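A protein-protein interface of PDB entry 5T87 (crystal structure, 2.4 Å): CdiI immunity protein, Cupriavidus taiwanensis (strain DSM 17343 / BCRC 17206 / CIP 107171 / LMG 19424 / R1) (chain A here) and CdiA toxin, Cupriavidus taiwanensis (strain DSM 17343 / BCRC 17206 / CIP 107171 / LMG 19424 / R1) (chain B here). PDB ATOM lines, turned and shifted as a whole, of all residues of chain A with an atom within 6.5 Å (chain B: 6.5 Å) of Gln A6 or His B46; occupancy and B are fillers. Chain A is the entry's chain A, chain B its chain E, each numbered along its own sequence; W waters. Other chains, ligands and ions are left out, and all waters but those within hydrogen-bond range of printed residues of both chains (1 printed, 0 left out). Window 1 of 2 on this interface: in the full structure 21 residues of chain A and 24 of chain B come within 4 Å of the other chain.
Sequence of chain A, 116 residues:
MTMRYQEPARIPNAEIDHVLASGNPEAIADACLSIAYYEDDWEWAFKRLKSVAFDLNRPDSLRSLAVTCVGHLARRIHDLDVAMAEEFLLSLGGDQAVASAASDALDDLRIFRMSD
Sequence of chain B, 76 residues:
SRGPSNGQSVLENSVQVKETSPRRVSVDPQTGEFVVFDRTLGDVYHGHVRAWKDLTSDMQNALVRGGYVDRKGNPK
The backbone carbonyl oxygen (O) of Arg A4 sits at hydrogen-bond distance from the backbone NH (N) of Tyr B45 (2.9 Å).
The backbone NH (N) of Gln A6 sits at hydrogen-bond distance from the backbone carbonyl oxygen (O) of Tyr B45.
OH of Tyr A37 is in hydrogen-bond range of O of Gly B47 (2.9 Å).
The backbone NH (N) of Tyr A5 lies within hydrogen-bond range of the side-chain amide oxygen (OE1) of Gln B8 (3.1 Å).
A ring nitrogen (NE2) of His A72 is in hydrogen-bond range of a ring nitrogen (NE2) of His B46 (3.2 Å).
The backbone NH of His B48 lies within hydrogen-bond range of the backbone carbonyl oxygen of Val B36, 3.0 Å away.
The backbone carbonyl oxygen of Leu A65 lies within hydrogen-bond range of the side-chain sulfur of Cys A69.
OG1 of Thr B40 is in hydrogen-bond range of ND1 of His B46 (2.8 Å).
O of His B46 sits at hydrogen-bond distance from N of Asp B38, 3.0 Å away.
C of Arg A4 touches CD2 of Leu B11 (3.5 Å).
N of Tyr A5 touches CD2 of Leu B11, at 3.4 Å.
Gly B47 touches Tyr A5.
Val B44 touches Gln A6.
Thr B40 touches Leu A33 (OG1 to CD1, 3.8 Å).
CD2 of Leu A33 touches CE1 of His B46, at 3.5 Å.
CD2 of His B46 touches OH of Tyr A37, 3.5 Å away.
Leu A65 touches Arg B39.
Leu A65 touches His B46 (CD1 to CE1, 3.8 Å).
CE1 of His A72 touches OD2 of Asp B38, at 3.4 Å.
Gln A6 touches three residues of chain B.
Of chain A, only Gln A6, Leu A33, Tyr A37, Leu A65 and His A72 come within 4 Å of His B46.
Of the printed residues of chain B, Leu A33 touches Thr B40 and His B46.
Printed residues of chain B within 4 Å of Tyr A5: Gln B8 (3.1 Å), Leu B11 (3.4 Å), Phe B37 (3.9 Å), Tyr B45 (3.5 Å) and Gly B47 (3.8 Å).
Printed residues of chain A within 4 Å of Val B44: Arg A4 (3.4 Å) and Gln A6 (3.8 Å).
Printed residues of chain A within 4 Å of Gln B8: Arg A4 and Tyr A5.
The nearest residue of chain A that does not touch His B46 is Pro A8 (4.02 Å).
The nearest printed residue of chain A that does not touch His B48 is Tyr A37 (4.03 Å).
Printed residues of chain B that touch a printed residue of chain A: Gln B8, Leu B11, Phe B37, Asp B38, Arg B39, Thr B40, Val B44, Tyr B45, His B46, Gly B47 and His B48.
Hydrophobic or aromatic side chains of chain B that line the printed part of chain A: Leu B11, Phe B37, Val B44, His B46 and His B48.
Hydrophobic or aromatic side chains of chain A that line the printed part of chain B: Tyr A5, Leu A33, Tyr A37, Leu A65 and His A72.
Among the printed residues, no Asp or Glu carboxylate lies within 4 Å of a Lys or Arg side-chain nitrogen of the other chain.
Water W1 bridges the side-chain hydroxyl (OG1) of Thr B40 (2.6 Å) and the backbone carbonyl oxygen (O) of Gln A6 (3.1 Å).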
ATOM      1  N   ARG A   4      -8.443  -8.153  20.276  1.00  0.00           N
ATOM      2  CA  ARG A   4      -9.838  -8.332  19.912  1.00  0.00           C
ATOM      3  C   ARG A   4     -10.683  -7.288  20.614  1.00  0.00           C
ATOM      4  O   ARG A   4     -10.615  -7.158  21.832  1.00  0.00           O
ATOM      5  CB  ARG A   4     -10.305  -9.727  20.319  1.00  0.00           C
ATOM      6  CG  ARG A   4      -9.751 -10.852  19.457  1.00  0.00           C
ATOM      7  CD  ARG A   4     -10.091 -12.206  20.056  1.00  0.00           C
ATOM      8  NE  ARG A   4      -9.280 -12.506  21.242  1.00  0.00           N
ATOM      9  CZ  ARG A   4      -9.555 -13.451  22.140  1.00  0.00           C
ATOM     10  NH1 ARG A   4     -10.647 -14.207  22.033  1.00  0.00           N
ATOM     11  NH2 ARG A   4      -8.734 -13.631  23.169  1.00  0.00           N
ATOM     12  N   TYR A   5     -11.474  -6.544  19.846  1.00  0.00           N
ATOM     13  CA  TYR A   5     -12.420  -5.586  20.394  1.00  0.00           C
ATOM     14  C   TYR A   5     -13.659  -6.337  20.850  1.00  0.00           C
ATOM     15  O   TYR A   5     -14.199  -7.128  20.097  1.00  0.00           O
ATOM     16  CB  TYR A   5     -12.814  -4.522  19.353  1.00  0.00           C
ATOM     17  CG  TYR A   5     -13.846  -3.527  19.866  1.00  0.00           C
ATOM     18  CD1 TYR A   5     -13.482  -2.516  20.755  1.00  0.00           C
ATOM     19  CD2 TYR A   5     -15.185  -3.616  19.483  1.00  0.00           C
ATOM     20  CE1 TYR A   5     -14.418  -1.611  21.243  1.00  0.00           C
ATOM     21  CE2 TYR A   5     -16.134  -2.718  19.961  1.00  0.00           C
ATOM     22  CZ  TYR A   5     -15.753  -1.714  20.846  1.00  0.00           C
ATOM     23  OH  TYR A   5     -16.687  -0.813  21.343  1.00  0.00           O
ATOM     24  N   GLN A   6     -14.091  -6.095  22.088  1.00  0.00           N
ATOM     25  CA  GLN A   6     -15.411  -6.540  22.548  1.00  0.00           C
ATOM     26  C   GLN A   6     -16.087  -5.386  23.270  1.00  0.00           C
ATOM     27  O   GLN A   6     -15.588  -4.881  24.279  1.00  0.00           O
ATOM     28  CB  GLN A   6     -15.335  -7.779  23.450  1.00  0.00           C
ATOM     29  CG  GLN A   6     -16.584  -8.671  23.397  1.00  0.00           C
ATOM     30  CD  GLN A   6     -16.430  -9.990  24.178  1.00  0.00           C
ATOM     31  OE1 GLN A   6     -15.748 -10.935  23.736  1.00  0.00           O
ATOM     32  NE2 GLN A   6     -17.077 -10.061  25.340  1.00  0.00           N
ATOM     33  N   GLU A   7     -17.203  -4.960  22.692  1.00  0.00           N
ATOM     34  CA  GLU A   7     -18.091  -4.007  23.295  1.00  0.00           C
ATOM     35  C   GLU A   7     -18.917  -4.752  24.333  1.00  0.00           C
ATOM     36  O   GLU A   7     -19.521  -5.771  24.012  1.00  0.00           O
ATOM     37  CB  GLU A   7     -19.012  -3.436  22.233  1.00  0.00           C
ATOM     38  CG  GLU A   7     -19.841  -2.250  22.687  1.00  0.00           C
ATOM     39  CD  GLU A   7     -20.355  -1.466  21.507  1.00  0.00           C
ATOM     40  OE1 GLU A   7     -20.722  -0.288  21.680  1.00  0.00           O
ATOM     41  OE2 GLU A   7     -20.365  -2.022  20.391  1.00  0.00           O
ATOM     42  N   PRO A   8     -18.947  -4.251  25.577  1.00  0.00           N
ATOM     43  CA  PRO A   8     -19.667  -4.908  26.666  1.00  0.00           C
ATOM     44  C   PRO A   8     -21.154  -5.184  26.413  1.00  0.00           C
ATOM     45  O   PRO A   8     -21.886  -4.290  25.990  1.00  0.00           O
ATOM     46  CB  PRO A   8     -19.535  -3.915  27.818  1.00  0.00           C
ATOM     47  CG  PRO A   8     -18.313  -3.130  27.523  1.00  0.00           C
ATOM     48  CD  PRO A   8     -18.146  -3.104  26.047  1.00  0.00           C
ATOM     49  N   ALA A   9     -21.578  -6.418  26.687  1.00  0.00           N
ATOM     50  CA  ALA A   9     -22.995  -6.788  26.679  1.00  0.00           C
ATOM     51  C   ALA A   9     -23.690  -6.203  27.896  1.00  0.00           C
ATOM     52  O   ALA A   9     -23.066  -6.017  28.936  1.00  0.00           O
ATOM     53  CB  ALA A   9     -23.147  -8.302  26.699  1.00  0.00           C
ATOM     54  N   ASP A  30     -17.603  -9.371  32.544  1.00  0.00           N
ATOM     55  CA  ASP A  30     -18.773  -8.890  31.836  1.00  0.00           C
ATOM     56  C   ASP A  30     -19.677  -8.112  32.763  1.00  0.00           C
ATOM     57  O   ASP A  30     -20.174  -7.075  32.388  1.00  0.00           O
ATOM     58  CB  ASP A  30     -19.548 -10.046  31.194  1.00  0.00           C
ATOM     59  CG  ASP A  30     -18.822 -10.651  30.016  1.00  0.00           C
ATOM     60  OD1 ASP A  30     -17.786 -10.099  29.588  1.00  0.00           O
ATOM     61  OD2 ASP A  30     -19.291 -11.700  29.531  1.00  0.00           O
ATOM     62  N   LEU A  33     -18.136  -4.765  33.591  1.00  0.00           N
ATOM     63  CA  LEU A  33     -18.282  -3.853  32.463  1.00  0.00           C
ATOM     64  C   LEU A  33     -19.724  -3.446  32.190  1.00  0.00           C
ATOM     65  O   LEU A  33     -19.967  -2.306  31.791  1.00  0.00           O
ATOM     66  CB  LEU A  33     -17.648  -4.427  31.215  1.00  0.00           C
ATOM     67  CG  LEU A  33     -16.128  -4.327  31.202  1.00  0.00           C
ATOM     68  CD1 LEU A  33     -15.595  -5.225  30.087  1.00  0.00           C
ATOM     69  CD2 LEU A  33     -15.649  -2.882  31.039  1.00  0.00           C
ATOM     70  N   TYR A  37     -20.607   0.488  32.006  1.00  0.00           N
ATOM     71  CA  TYR A  37     -21.143   1.126  30.794  1.00  0.00           C
ATOM     72  C   TYR A  37     -22.621   1.476  30.857  1.00  0.00           C
ATOM     73  O   TYR A  37     -23.040   2.423  30.195  1.00  0.00           O
ATOM     74  CB  TYR A  37     -20.901   0.241  29.530  1.00  0.00           C
ATOM     75  CG  TYR A  37     -19.558   0.420  28.842  1.00  0.00           C
ATOM     76  CD1 TYR A  37     -18.399   0.596  29.588  1.00  0.00           C
ATOM     77  CD2 TYR A  37     -19.441   0.367  27.437  1.00  0.00           C
ATOM     78  CE1 TYR A  37     -17.167   0.747  28.976  1.00  0.00           C
ATOM     79  CE2 TYR A  37     -18.195   0.499  26.810  1.00  0.00           C
ATOM     80  CZ  TYR A  37     -17.058   0.697  27.596  1.00  0.00           C
ATOM     81  OH  TYR A  37     -15.791   0.872  27.085  1.00  0.00           O
ATOM     82  N   LEU A  65      -9.434  -4.688  36.696  1.00  0.00           N
ATOM     83  CA  LEU A  65     -10.529  -4.326  35.801  1.00  0.00           C
ATOM     84  C   LEU A  65     -11.637  -3.540  36.540  1.00  0.00           C
ATOM     85  O   LEU A  65     -12.169  -2.530  36.036  1.00  0.00           O
ATOM     86  CB  LEU A  65     -11.112  -5.576  35.131  1.00  0.00           C
ATOM     87  CG  LEU A  65     -12.353  -5.327  34.262  1.00  0.00           C
ATOM     88  CD1 LEU A  65     -12.033  -4.347  33.157  1.00  0.00           C
ATOM     89  CD2 LEU A  65     -12.926  -6.611  33.699  1.00  0.00           C
ATOM     90  N   THR A  68     -10.612   0.001  36.925  1.00  0.00           N
ATOM     91  CA  THR A  68     -10.819   0.634  35.628  1.00  0.00           C
ATOM     92  C   THR A  68     -12.305   0.933  35.406  1.00  0.00           C
ATOM     93  O   THR A  68     -12.659   2.018  34.951  1.00  0.00           O
ATOM     94  CB  THR A  68     -10.204  -0.239  34.499  1.00  0.00           C
ATOM     95  OG1 THR A  68      -8.784  -0.072  34.517  1.00  0.00           O
ATOM     96  CG2 THR A  68     -10.721   0.132  33.110  1.00  0.00           C
ATOM     97  N   CYS A  69     -13.161  -0.017  35.762  1.00  0.00           N
ATOM     98  CA  CYS A  69     -14.609   0.192  35.715  1.00  0.00           C
ATOM     99  C   CYS A  69     -15.099   1.337  36.607  1.00  0.00           C
ATOM    100  O   CYS A  69     -16.030   2.058  36.235  1.00  0.00           O
ATOM    101  CB  CYS A  69     -15.350  -1.093  36.074  1.00  0.00           C
ATOM    102  SG  CYS A  69     -15.326  -2.271  34.719  1.00  0.00           S
ATOM    103  N   HIS A  72     -14.677   4.283  34.683  1.00  0.00           N
ATOM    104  CA  HIS A  72     -15.735   4.453  33.696  1.00  0.00           C
ATOM    105  C   HIS A  72     -16.966   5.069  34.303  1.00  0.00           C
ATOM    106  O   HIS A  72     -17.552   5.977  33.702  1.00  0.00           O
ATOM    107  CB  HIS A  72     -16.106   3.128  33.030  1.00  0.00           C
ATOM    108  CG  HIS A  72     -15.002   2.543  32.223  1.00  0.00           C
ATOM    109  ND1 HIS A  72     -14.178   3.309  31.430  1.00  0.00           N
ATOM    110  CD2 HIS A  72     -14.576   1.268  32.088  1.00  0.00           C
ATOM    111  CE1 HIS A  72     -13.293   2.532  30.834  1.00  0.00           C
ATOM    112  NE2 HIS A  72     -13.509   1.289  31.222  1.00  0.00           N
ATOM    113  N   GLN B   8     -12.716  -2.903  15.848  1.00  0.00           N
ATOM    114  CA  GLN B   8     -11.637  -3.865  15.610  1.00  0.00           C
ATOM    115  C   GLN B   8     -10.406  -3.228  14.933  1.00  0.00           C
ATOM    116  O   GLN B   8      -9.296  -3.313  15.470  1.00  0.00           O
ATOM    117  CB  GLN B   8     -12.167  -5.078  14.827  1.00  0.00           C
ATOM    118  CG  GLN B   8     -11.218  -6.263  14.723  1.00  0.00           C
ATOM    119  CD  GLN B   8     -10.733  -6.757  16.073  1.00  0.00           C
ATOM    120  OE1 GLN B   8     -11.511  -7.263  16.874  1.00  0.00           O
ATOM    121  NE2 GLN B   8      -9.444  -6.614  16.328  1.00  0.00           N
ATOM    122  N   LEU B  11      -8.716  -0.438  17.034  1.00  0.00           N
ATOM    123  CA  LEU B  11      -7.911  -1.100  18.073  1.00  0.00           C
ATOM    124  C   LEU B  11      -6.570  -1.599  17.538  1.00  0.00           C
ATOM    125  O   LEU B  11      -5.541  -1.374  18.171  1.00  0.00           O
ATOM    126  CB  LEU B  11      -8.691  -2.270  18.701  1.00  0.00           C
ATOM    127  CG  LEU B  11      -8.005  -3.194  19.727  1.00  0.00           C
ATOM    128  CD1 LEU B  11      -7.410  -2.411  20.883  1.00  0.00           C
ATOM    129  CD2 LEU B  11      -8.994  -4.232  20.242  1.00  0.00           C
ATOM    130  N   VAL B  36     -10.391   5.652  23.363  1.00  0.00           N
ATOM    131  CA  VAL B  36      -9.602   5.089  24.466  1.00  0.00           C
ATOM    132  C   VAL B  36      -9.990   3.622  24.667  1.00  0.00           C
ATOM    133  O   VAL B  36     -11.183   3.294  24.773  1.00  0.00           O
ATOM    134  CB  VAL B  36      -9.858   5.844  25.783  1.00  0.00           C
ATOM    135  CG1 VAL B  36      -9.098   5.196  26.946  1.00  0.00           C
ATOM    136  CG2 VAL B  36      -9.495   7.318  25.656  1.00  0.00           C
ATOM    137  N   PHE B  37      -8.970   2.762  24.740  1.00  0.00           N
ATOM    138  CA  PHE B  37      -9.141   1.318  24.885  1.00  0.00           C
ATOM    139  C   PHE B  37      -8.509   0.824  26.161  1.00  0.00           C
ATOM    140  O   PHE B  37      -7.389   1.207  26.475  1.00  0.00           O
ATOM    141  CB  PHE B  37      -8.440   0.602  23.741  1.00  0.00           C
ATOM    142  CG  PHE B  37      -9.075   0.824  22.409  1.00  0.00           C
ATOM    143  CD1 PHE B  37     -10.264   0.176  22.081  1.00  0.00           C
ATOM    144  CD2 PHE B  37      -8.480   1.659  21.465  1.00  0.00           C
ATOM    145  CE1 PHE B  37     -10.864   0.371  20.845  1.00  0.00           C
ATOM    146  CE2 PHE B  37      -9.069   1.848  20.220  1.00  0.00           C
ATOM    147  CZ  PHE B  37     -10.265   1.201  19.913  1.00  0.00           C
ATOM    148  N   ASP B  38      -9.202  -0.071  26.856  1.00  0.00           N
ATOM    149  CA  ASP B  38      -8.699  -0.662  28.096  1.00  0.00           C
ATOM    150  C   ASP B  38      -8.810  -2.167  28.037  1.00  0.00           C
ATOM    151  O   ASP B  38      -9.704  -2.704  27.386  1.00  0.00           O
ATOM    152  CB  ASP B  38      -9.511  -0.160  29.284  1.00  0.00           C
ATOM    153  CG  ASP B  38      -9.462   1.338  29.425  1.00  0.00           C
ATOM    154  OD1 ASP B  38      -8.413   1.839  29.889  1.00  0.00           O
ATOM    155  OD2 ASP B  38     -10.457   2.009  29.046  1.00  0.00           O
ATOM    156  N   ARG B  39      -7.920  -2.847  28.745  1.00  0.00           N
ATOM    157  CA  ARG B  39      -7.927  -4.290  28.752  1.00  0.00           C
ATOM    158  C   ARG B  39      -9.138  -4.829  29.499  1.00  0.00           C
ATOM    159  O   ARG B  39      -9.483  -4.334  30.563  1.00  0.00           O
ATOM    160  CB  ARG B  39      -6.671  -4.861  29.399  1.00  0.00           C
ATOM    161  CG  ARG B  39      -6.467  -6.319  29.007  1.00  0.00           C
ATOM    162  CD  ARG B  39      -5.608  -7.051  29.996  1.00  0.00           C
ATOM    163  NE  ARG B  39      -4.204  -6.715  29.803  1.00  0.00           N
ATOM    164  CZ  ARG B  39      -3.290  -6.620  30.774  1.00  0.00           C
ATOM    165  NH1 ARG B  39      -3.609  -6.821  32.059  1.00  0.00           N
ATOM    166  NH2 ARG B  39      -2.039  -6.312  30.453  1.00  0.00           N
ATOM    167  N   THR B  40      -9.763  -5.850  28.930  1.00  0.00           N
ATOM    168  CA  THR B  40     -10.802  -6.581  29.600  1.00  0.00           C
ATOM    169  C   THR B  40     -10.125  -7.753  30.304  1.00  0.00           C
ATOM    170  O   THR B  40     -10.068  -7.805  31.529  1.00  0.00           O
ATOM    171  CB  THR B  40     -11.870  -7.022  28.577  1.00  0.00           C
ATOM    172  OG1 THR B  40     -12.455  -5.857  27.968  1.00  0.00           O
ATOM    173  CG2 THR B  40     -12.949  -7.893  29.210  1.00  0.00           C
ATOM    174  N   LEU B  41      -9.590  -8.667  29.509  1.00  0.00           N
ATOM    175  CA  LEU B  41      -8.909  -9.884  29.956  1.00  0.00           C
ATOM    176  C   LEU B  41      -8.083 -10.348  28.746  1.00  0.00           C
ATOM    177  O   LEU B  41      -8.534 -10.204  27.612  1.00  0.00           O
ATOM    178  CB  LEU B  41      -9.918 -10.977  30.341  1.00  0.00           C
ATOM    179  CG  LEU B  41     -10.668 -10.908  31.679  1.00  0.00           C
ATOM    180  CD1 LEU B  41     -11.646 -12.067  31.884  1.00  0.00           C
ATOM    181  CD2 LEU B  41      -9.678 -10.837  32.838  1.00  0.00           C
ATOM    182  N   VAL B  44      -8.160  -9.189  24.915  1.00  0.00           N
ATOM    183  CA  VAL B  44      -9.470  -8.553  24.660  1.00  0.00           C
ATOM    184  C   VAL B  44      -9.537  -7.149  25.277  1.00  0.00           C
ATOM    185  O   VAL B  44      -9.084  -6.949  26.402  1.00  0.00           O
ATOM    186  CB  VAL B  44     -10.639  -9.384  25.230  1.00  0.00           C
ATOM    187  CG1 VAL B  44     -11.985  -8.700  24.973  1.00  0.00           C
ATOM    188  CG2 VAL B  44     -10.611 -10.795  24.656  1.00  0.00           C
ATOM    189  N   TYR B  45     -10.106  -6.202  24.528  1.00  0.00           N
ATOM    190  CA  TYR B  45     -10.193  -4.799  24.926  1.00  0.00           C
ATOM    191  C   TYR B  45     -11.610  -4.244  24.704  1.00  0.00           C
ATOM    192  O   TYR B  45     -12.304  -4.683  23.769  1.00  0.00           O
ATOM    193  CB  TYR B  45      -9.189  -3.961  24.123  1.00  0.00           C
ATOM    194  CG  TYR B  45      -7.734  -4.149  24.527  1.00  0.00           C
ATOM    195  CD1 TYR B  45      -7.009  -5.268  24.124  1.00  0.00           C
ATOM    196  CD2 TYR B  45      -7.070  -3.189  25.291  1.00  0.00           C
ATOM    197  CE1 TYR B  45      -5.675  -5.437  24.490  1.00  0.00           C
ATOM    198  CE2 TYR B  45      -5.742  -3.344  25.661  1.00  0.00           C
ATOM    199  CZ  TYR B  45      -5.048  -4.461  25.261  1.00  0.00           C
ATOM    200  OH  TYR B  45      -3.739  -4.571  25.639  1.00  0.00           O
ATOM    201  N   HIS B  46     -12.018  -3.294  25.557  1.00  0.00           N
ATOM    202  CA  HIS B  46     -13.243  -2.469  25.353  1.00  0.00           C
ATOM    203  C   HIS B  46     -12.846  -1.011  25.123  1.00  0.00           C
ATOM    204  O   HIS B  46     -11.700  -0.630  25.373  1.00  0.00           O
ATOM    205  CB  HIS B  46     -14.196  -2.533  26.555  1.00  0.00           C
ATOM    206  CG  HIS B  46     -13.527  -2.244  27.862  1.00  0.00           C
ATOM    207  ND1 HIS B  46     -12.972  -3.238  28.637  1.00  0.00           N
ATOM    208  CD2 HIS B  46     -13.274  -1.080  28.504  1.00  0.00           C
ATOM    209  CE1 HIS B  46     -12.431  -2.705  29.715  1.00  0.00           C
ATOM    210  NE2 HIS B  46     -12.605  -1.400  29.661  1.00  0.00           N
ATOM    211  N   GLY B  47     -13.785  -0.194  24.662  1.00  0.00           N
ATOM    212  CA  GLY B  47     -13.440   1.179  24.329  1.00  0.00           C
ATOM    213  C   GLY B  47     -14.560   2.185  24.393  1.00  0.00           C
ATOM    214  O   GLY B  47     -15.753   1.825  24.383  1.00  0.00           O
ATOM    215  N   HIS B  48     -14.160   3.455  24.462  1.00  0.00           N
ATOM    216  CA  HIS B  48     -15.113   4.567  24.482  1.00  0.00           C
ATOM    217  C   HIS B  48     -14.599   5.750  23.690  1.00  0.00           C
ATOM    218  O   HIS B  48     -13.387   5.904  23.505  1.00  0.00           O
ATOM    219  CB  HIS B  48     -15.454   4.990  25.926  1.00  0.00           C
ATOM    220  CG  HIS B  48     -14.274   5.451  26.722  1.00  0.00           C
ATOM    221  ND1 HIS B  48     -13.555   4.606  27.537  1.00  0.00           N
ATOM    222  CD2 HIS B  48     -13.691   6.667  26.834  1.00  0.00           C
ATOM    223  CE1 HIS B  48     -12.574   5.277  28.112  1.00  0.00           C
ATOM    224  NE2 HIS B  48     -12.631   6.528  27.697  1.00  0.00           N
HETATM  225  O   HOH W   1     -14.601  -6.496  26.686  1.00  0.00           O
